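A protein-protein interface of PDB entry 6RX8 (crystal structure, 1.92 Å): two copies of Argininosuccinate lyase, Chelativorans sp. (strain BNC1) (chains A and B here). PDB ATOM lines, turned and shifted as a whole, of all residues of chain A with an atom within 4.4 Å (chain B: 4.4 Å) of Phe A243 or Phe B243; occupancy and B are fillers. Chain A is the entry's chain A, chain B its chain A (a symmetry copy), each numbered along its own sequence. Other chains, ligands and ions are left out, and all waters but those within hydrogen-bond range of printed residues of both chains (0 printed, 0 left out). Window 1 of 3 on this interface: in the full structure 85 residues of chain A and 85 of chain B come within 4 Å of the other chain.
Hydrophobic or aromatic side chains of chain B that line the printed part of chain A: Ala B239, Phe B243, Val B247, Leu B306 and Leu B310.
Hydrophobic or aromatic side chains of chain A within 4 Å of the printed part of chain B: Ala A239, Phe A243, Val A247, Leu A306 and Leu A310.
Among the printed residues, no Asp or Glu carboxylate lies within 4 Å of a Lys or Arg side-chain nitrogen of the other chain.
Ala A239 touches Val B247, and with the chains exchanged Val A247 touches Ala B239.
Glu A240 touches Phe B243, and with the chains exchanged Phe A243 touches Glu B240.
Phe B243 touches its own counterpart, Phe A243.
Leu A306 touches Leu B310, and with the chains exchanged Leu A310 touches Leu B306.
11 positions are printed for both chains.
Of the 11 pairs that touch across the chains among the printed residues, 11 have their exchanged pair printed and touching as well.
CE1 of Phe B243 touches O of Ala A239 (3.7 Å).
Ala A239 touches Val B247.
Glu A240 touches Phe B243 (CA to CZ, 3.4 Å).
CZ of Phe A243 touches CA of Glu B240 (3.4 Å).
Phe B243 touches Phe A243.
Ala B239 touches Val A247.
CD2 of Leu B310 touches CA of Val A247, 3.9 Å away.
CD1 of Leu B310 touches CD2 of Leu A306 (3.4 Å).
Val B247 touches Leu A310 (CA to CD2, 3.9 Å).
Leu A310 touches Leu B306 (CD1 to CD2, 3.4 Å).
His A241 touches none of the printed residues of chain B.
Of chain B, only Ala B239 (3.7 Å), Glu B240 (3.4 Å) and Phe B243 (3.4 Å) come within 4 Å of Phe A243.
Printed residues of chain B within 4 Å of Val A247: Ala B239 (3.9 Å) and Leu B310 (3.9 Å).
Of the printed residues of chain B, Leu A306 touches Leu B310 (3.4 Å).
His B241 touches none of the printed residues of chain A.
Phe B243 touches three residues of chain A.
Printed residues of chain A within 4 Å of Leu B306: Leu A310.
Of the printed residues of chain A, Leu B310 touches Val A247 and Leu A306.
The nearest residue of chain B that does not touch Phe A243 is Leu B306 (4.04 Å).
The nearest residue of chain A that does not touch Phe B243 is Leu A306 (4.04 Å).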
ATOM      1  N   ALA A 239      10.371 -10.337 -11.014  1.00  0.00           N
ATOM      2  CA  ALA A 239      10.862 -11.284 -12.003  1.00  0.00           C
ATOM      3  C   ALA A 239      10.410 -10.892 -13.401  1.00  0.00           C
ATOM      4  O   ALA A 239      11.192 -10.957 -14.359  1.00  0.00           O
ATOM      5  CB  ALA A 239      10.372 -12.688 -11.656  1.00  0.00           C
ATOM      6  N   GLU A 240       9.146 -10.487 -13.541  1.00  0.00           N
ATOM      7  CA  GLU A 240       8.625 -10.155 -14.859  1.00  0.00           C
ATOM      8  C   GLU A 240       9.299  -8.904 -15.401  1.00  0.00           C
ATOM      9  O   GLU A 240       9.644  -8.839 -16.585  1.00  0.00           O
ATOM     10  CB  GLU A 240       7.113  -9.973 -14.793  1.00  0.00           C
ATOM     11  CG  GLU A 240       6.489  -9.715 -16.151  1.00  0.00           C
ATOM     12  CD  GLU A 240       4.988  -9.588 -16.079  1.00  0.00           C
ATOM     13  OE1 GLU A 240       4.420  -9.804 -14.990  1.00  0.00           O
ATOM     14  OE2 GLU A 240       4.381  -9.268 -17.117  1.00  0.00           O
ATOM     15  N   HIS A 241       9.516  -7.910 -14.541  1.00  0.00           N
ATOM     16  CA  HIS A 241      10.253  -6.723 -14.951  1.00  0.00           C
ATOM     17  C   HIS A 241      11.628  -7.108 -15.472  1.00  0.00           C
ATOM     18  O   HIS A 241      12.067  -6.635 -16.527  1.00  0.00           O
ATOM     19  CB  HIS A 241      10.379  -5.762 -13.772  1.00  0.00           C
ATOM     20  CG  HIS A 241      10.730  -4.363 -14.171  1.00  0.00           C
ATOM     21  ND1 HIS A 241      10.395  -3.269 -13.406  1.00  0.00           N
ATOM     22  CD2 HIS A 241      11.381  -3.882 -15.256  1.00  0.00           C
ATOM     23  CE1 HIS A 241      10.822  -2.172 -14.004  1.00  0.00           C
ATOM     24  NE2 HIS A 241      11.428  -2.516 -15.126  1.00  0.00           N
ATOM     25  N   ALA A 242      12.318  -7.989 -14.750  1.00  0.00           N
ATOM     26  CA  ALA A 242      13.636  -8.414 -15.186  1.00  0.00           C
ATOM     27  C   ALA A 242      13.547  -9.178 -16.494  1.00  0.00           C
ATOM     28  O   ALA A 242      14.421  -9.045 -17.357  1.00  0.00           O
ATOM     29  CB  ALA A 242      14.298  -9.269 -14.107  1.00  0.00           C
ATOM     30  N   PHE A 243      12.491  -9.973 -16.668  1.00  0.00           N
ATOM     31  CA  PHE A 243      12.382 -10.731 -17.899  1.00  0.00           C
ATOM     32  C   PHE A 243      12.135  -9.826 -19.099  1.00  0.00           C
ATOM     33  O   PHE A 243      12.754  -9.999 -20.154  1.00  0.00           O
ATOM     34  CB  PHE A 243      11.270 -11.754 -17.848  1.00  0.00           C
ATOM     35  CG  PHE A 243      10.925 -12.263 -19.203  1.00  0.00           C
ATOM     36  CD1 PHE A 243      11.808 -13.101 -19.867  1.00  0.00           C
ATOM     37  CD2 PHE A 243       9.784 -11.831 -19.859  1.00  0.00           C
ATOM     38  CE1 PHE A 243      11.537 -13.550 -21.141  1.00  0.00           C
ATOM     39  CE2 PHE A 243       9.493 -12.281 -21.137  1.00  0.00           C
ATOM     40  CZ  PHE A 243      10.375 -13.146 -21.783  1.00  0.00           C
ATOM     41  N   VAL A 244      11.181  -8.896 -18.991  1.00  0.00           N
ATOM     42  CA  VAL A 244      10.890  -8.071 -20.157  1.00  0.00           C
ATOM     43  C   VAL A 244      12.122  -7.262 -20.528  1.00  0.00           C
ATOM     44  O   VAL A 244      12.449  -7.107 -21.710  1.00  0.00           O
ATOM     45  CB  VAL A 244       9.665  -7.175 -19.921  1.00  0.00           C
ATOM     46  CG1 VAL A 244       9.384  -6.350 -21.178  1.00  0.00           C
ATOM     47  CG2 VAL A 244       8.448  -8.020 -19.591  1.00  0.00           C
ATOM     48  N   ASN A 245      12.847  -6.760 -19.527  1.00  0.00           N
ATOM     49  CA  ASN A 245      14.118  -6.101 -19.805  1.00  0.00           C
ATOM     50  C   ASN A 245      15.038  -7.016 -20.602  1.00  0.00           C
ATOM     51  O   ASN A 245      15.671  -6.596 -21.579  1.00  0.00           O
ATOM     52  CB  ASN A 245      14.800  -5.706 -18.497  1.00  0.00           C
ATOM     53  CG  ASN A 245      14.173  -4.496 -17.827  1.00  0.00           C
ATOM     54  OD1 ASN A 245      13.156  -3.950 -18.275  1.00  0.00           O
ATOM     55  ND2 ASN A 245      14.793  -4.069 -16.733  1.00  0.00           N
ATOM     56  N   ALA A 246      15.154  -8.267 -20.166  1.00  0.00           N
ATOM     57  CA  ALA A 246      16.084  -9.194 -20.798  1.00  0.00           C
ATOM     58  C   ALA A 246      15.663  -9.501 -22.226  1.00  0.00           C
ATOM     59  O   ALA A 246      16.495  -9.484 -23.142  1.00  0.00           O
ATOM     60  CB  ALA A 246      16.169 -10.473 -19.973  1.00  0.00           C
ATOM     61  N   VAL A 247      14.376  -9.776 -22.445  1.00  0.00           N
ATOM     62  CA  VAL A 247      13.956 -10.163 -23.786  1.00  0.00           C
ATOM     63  C   VAL A 247      13.958  -8.947 -24.704  1.00  0.00           C
ATOM     64  O   VAL A 247      14.414  -9.023 -25.849  1.00  0.00           O
ATOM     65  CB  VAL A 247      12.591 -10.874 -23.765  1.00  0.00           C
ATOM     66  CG1 VAL A 247      11.442  -9.917 -23.537  1.00  0.00           C
ATOM     67  CG2 VAL A 247      12.392 -11.662 -25.086  1.00  0.00           C
ATOM     68  N   LEU A 306      17.496 -11.425 -13.877  1.00  0.00           N
ATOM     69  CA  LEU A 306      16.413 -12.365 -14.142  1.00  0.00           C
ATOM     70  C   LEU A 306      16.690 -13.709 -13.485  1.00  0.00           C
ATOM     71  O   LEU A 306      15.827 -14.276 -12.806  1.00  0.00           O
ATOM     72  CB  LEU A 306      16.240 -12.522 -15.652  1.00  0.00           C
ATOM     73  CG  LEU A 306      15.234 -13.566 -16.137  1.00  0.00           C
ATOM     74  CD1 LEU A 306      13.834 -13.205 -15.695  1.00  0.00           C
ATOM     75  CD2 LEU A 306      15.333 -13.689 -17.659  1.00  0.00           C
ATOM     76  N   LEU A 310      14.668 -15.154 -10.095  1.00  0.00           N
ATOM     77  CA  LEU A 310      13.932 -16.408 -10.189  1.00  0.00           C
ATOM     78  C   LEU A 310      14.559 -17.474  -9.301  1.00  0.00           C
ATOM     79  O   LEU A 310      13.849 -18.280  -8.685  1.00  0.00           O
ATOM     80  CB  LEU A 310      13.883 -16.885 -11.638  1.00  0.00           C
ATOM     81  CG  LEU A 310      12.872 -16.196 -12.555  1.00  0.00           C
ATOM     82  CD1 LEU A 310      13.123 -16.643 -14.000  1.00  0.00           C
ATOM     83  CD2 LEU A 310      11.437 -16.500 -12.118  1.00  0.00           C
ATOM     84  N   ALA B 239      10.732 -17.228 -25.778  1.00  0.00           N
ATOM     85  CA  ALA B 239      11.329 -16.782 -24.529  1.00  0.00           C
ATOM     86  C   ALA B 239      10.257 -16.472 -23.496  1.00  0.00           C
ATOM     87  O   ALA B 239      10.392 -16.830 -22.319  1.00  0.00           O
ATOM     88  CB  ALA B 239      12.197 -15.553 -24.786  1.00  0.00           C
ATOM     89  N   GLU B 240       9.183 -15.800 -23.916  1.00  0.00           N
ATOM     90  CA  GLU B 240       8.146 -15.413 -22.972  1.00  0.00           C
ATOM     91  C   GLU B 240       7.419 -16.640 -22.442  1.00  0.00           C
ATOM     92  O   GLU B 240       7.125 -16.728 -21.247  1.00  0.00           O
ATOM     93  CB  GLU B 240       7.168 -14.448 -23.634  1.00  0.00           C
ATOM     94  CG  GLU B 240       6.110 -13.930 -22.680  1.00  0.00           C
ATOM     95  CD  GLU B 240       5.183 -12.938 -23.333  1.00  0.00           C
ATOM     96  OE1 GLU B 240       5.424 -12.571 -24.501  1.00  0.00           O
ATOM     97  OE2 GLU B 240       4.210 -12.529 -22.674  1.00  0.00           O
ATOM     98  N   HIS B 241       7.148 -17.609 -23.315  1.00  0.00           N
ATOM     99  CA  HIS B 241       6.555 -18.862 -22.871  1.00  0.00           C
ATOM    100  C   HIS B 241       7.429 -19.513 -21.811  1.00  0.00           C
ATOM    101  O   HIS B 241       6.939 -19.963 -20.768  1.00  0.00           O
ATOM    102  CB  HIS B 241       6.375 -19.798 -24.063  1.00  0.00           C
ATOM    103  CG  HIS B 241       5.411 -20.914 -23.811  1.00  0.00           C
ATOM    104  ND1 HIS B 241       4.712 -21.532 -24.824  1.00  0.00           N
ATOM    105  CD2 HIS B 241       5.026 -21.518 -22.662  1.00  0.00           C
ATOM    106  CE1 HIS B 241       3.935 -22.467 -24.309  1.00  0.00           C
ATOM    107  NE2 HIS B 241       4.110 -22.484 -23.001  1.00  0.00           N
ATOM    108  N   ALA B 242       8.738 -19.554 -22.055  1.00  0.00           N
ATOM    109  CA  ALA B 242       9.640 -20.152 -21.086  1.00  0.00           C
ATOM    110  C   ALA B 242       9.649 -19.352 -19.798  1.00  0.00           C
ATOM    111  O   ALA B 242       9.729 -19.925 -18.706  1.00  0.00           O
ATOM    112  CB  ALA B 242      11.047 -20.252 -21.669  1.00  0.00           C
ATOM    113  N   PHE B 243       9.553 -18.026 -19.899  1.00  0.00           N
ATOM    114  CA  PHE B 243       9.577 -17.228 -18.688  1.00  0.00           C
ATOM    115  C   PHE B 243       8.324 -17.442 -17.848  1.00  0.00           C
ATOM    116  O   PHE B 243       8.408 -17.593 -16.624  1.00  0.00           O
ATOM    117  CB  PHE B 243       9.699 -15.749 -18.977  1.00  0.00           C
ATOM    118  CG  PHE B 243       9.359 -14.924 -17.786  1.00  0.00           C
ATOM    119  CD1 PHE B 243      10.224 -14.892 -16.704  1.00  0.00           C
ATOM    120  CD2 PHE B 243       8.141 -14.269 -17.695  1.00  0.00           C
ATOM    121  CE1 PHE B 243       9.914 -14.175 -15.569  1.00  0.00           C
ATOM    122  CE2 PHE B 243       7.819 -13.536 -16.564  1.00  0.00           C
ATOM    123  CZ  PHE B 243       8.710 -13.489 -15.493  1.00  0.00           C
ATOM    124  N   VAL B 244       7.142 -17.387 -18.468  1.00  0.00           N
ATOM    125  CA  VAL B 244       5.935 -17.522 -17.661  1.00  0.00           C
ATOM    126  C   VAL B 244       5.916 -18.891 -16.999  1.00  0.00           C
ATOM    127  O   VAL B 244       5.545 -19.025 -15.828  1.00  0.00           O
ATOM    128  CB  VAL B 244       4.669 -17.270 -18.493  1.00  0.00           C
ATOM    129  CG1 VAL B 244       3.435 -17.396 -17.600  1.00  0.00           C
ATOM    130  CG2 VAL B 244       4.708 -15.882 -19.106  1.00  0.00           C
ATOM    131  N   ASN B 245       6.346 -19.925 -17.723  1.00  0.00           N
ATOM    132  CA  ASN B 245       6.494 -21.237 -17.106  1.00  0.00           C
ATOM    133  C   ASN B 245       7.386 -21.158 -15.875  1.00  0.00           C
ATOM    134  O   ASN B 245       7.076 -21.727 -14.820  1.00  0.00           O
ATOM    135  CB  ASN B 245       7.093 -22.223 -18.106  1.00  0.00           C
ATOM    136  CG  ASN B 245       6.107 -22.689 -19.163  1.00  0.00           C
ATOM    137  OD1 ASN B 245       4.957 -22.236 -19.235  1.00  0.00           O
ATOM    138  ND2 ASN B 245       6.566 -23.614 -19.999  1.00  0.00           N
ATOM    139  N   ALA B 246       8.526 -20.486 -16.009  1.00  0.00           N
ATOM    140  CA  ALA B 246       9.494 -20.434 -14.923  1.00  0.00           C
ATOM    141  C   ALA B 246       8.936 -19.676 -13.729  1.00  0.00           C
ATOM    142  O   ALA B 246       9.056 -20.131 -12.585  1.00  0.00           O
ATOM    143  CB  ALA B 246      10.783 -19.788 -15.418  1.00  0.00           C
ATOM    144  N   VAL B 247       8.314 -18.521 -13.967  1.00  0.00           N
ATOM    145  CA  VAL B 247       7.847 -17.724 -12.839  1.00  0.00           C
ATOM    146  C   VAL B 247       6.619 -18.375 -12.215  1.00  0.00           C
ATOM    147  O   VAL B 247       6.505 -18.457 -10.988  1.00  0.00           O
ATOM    148  CB  VAL B 247       7.586 -16.264 -13.249  1.00  0.00           C
ATOM    149  CG1 VAL B 247       6.318 -16.106 -14.057  1.00  0.00           C
ATOM    150  CG2 VAL B 247       7.545 -15.366 -11.986  1.00  0.00           C
ATOM    151  N   LEU B 306      14.538 -21.179 -20.296  1.00  0.00           N
ATOM    152  CA  LEU B 306      14.498 -19.721 -20.300  1.00  0.00           C
ATOM    153  C   LEU B 306      15.881 -19.142 -20.559  1.00  0.00           C
ATOM    154  O   LEU B 306      16.053 -18.257 -21.404  1.00  0.00           O
ATOM    155  CB  LEU B 306      13.943 -19.229 -18.965  1.00  0.00           C
ATOM    156  CG  LEU B 306      13.939 -17.719 -18.722  1.00  0.00           C
ATOM    157  CD1 LEU B 306      13.039 -17.020 -19.715  1.00  0.00           C
ATOM    158  CD2 LEU B 306      13.511 -17.444 -17.279  1.00  0.00           C
ATOM    159  N   LEU B 310      17.047 -17.303 -24.155  1.00  0.00           N
ATOM    160  CA  LEU B 310      17.499 -15.917 -24.129  1.00  0.00           C
ATOM    161  C   LEU B 310      18.968 -15.818 -24.515  1.00  0.00           C
ATOM    162  O   LEU B 310      19.378 -14.874 -25.202  1.00  0.00           O
ATOM    163  CB  LEU B 310      17.270 -15.313 -22.747  1.00  0.00           C
ATOM    164  CG  LEU B 310      15.842 -14.877 -22.414  1.00  0.00           C
ATOM    165  CD1 LEU B 310      15.766 -14.511 -20.927  1.00  0.00           C
ATOM    166  CD2 LEU B 310      15.403 -13.710 -23.300  1.00  0.00           C
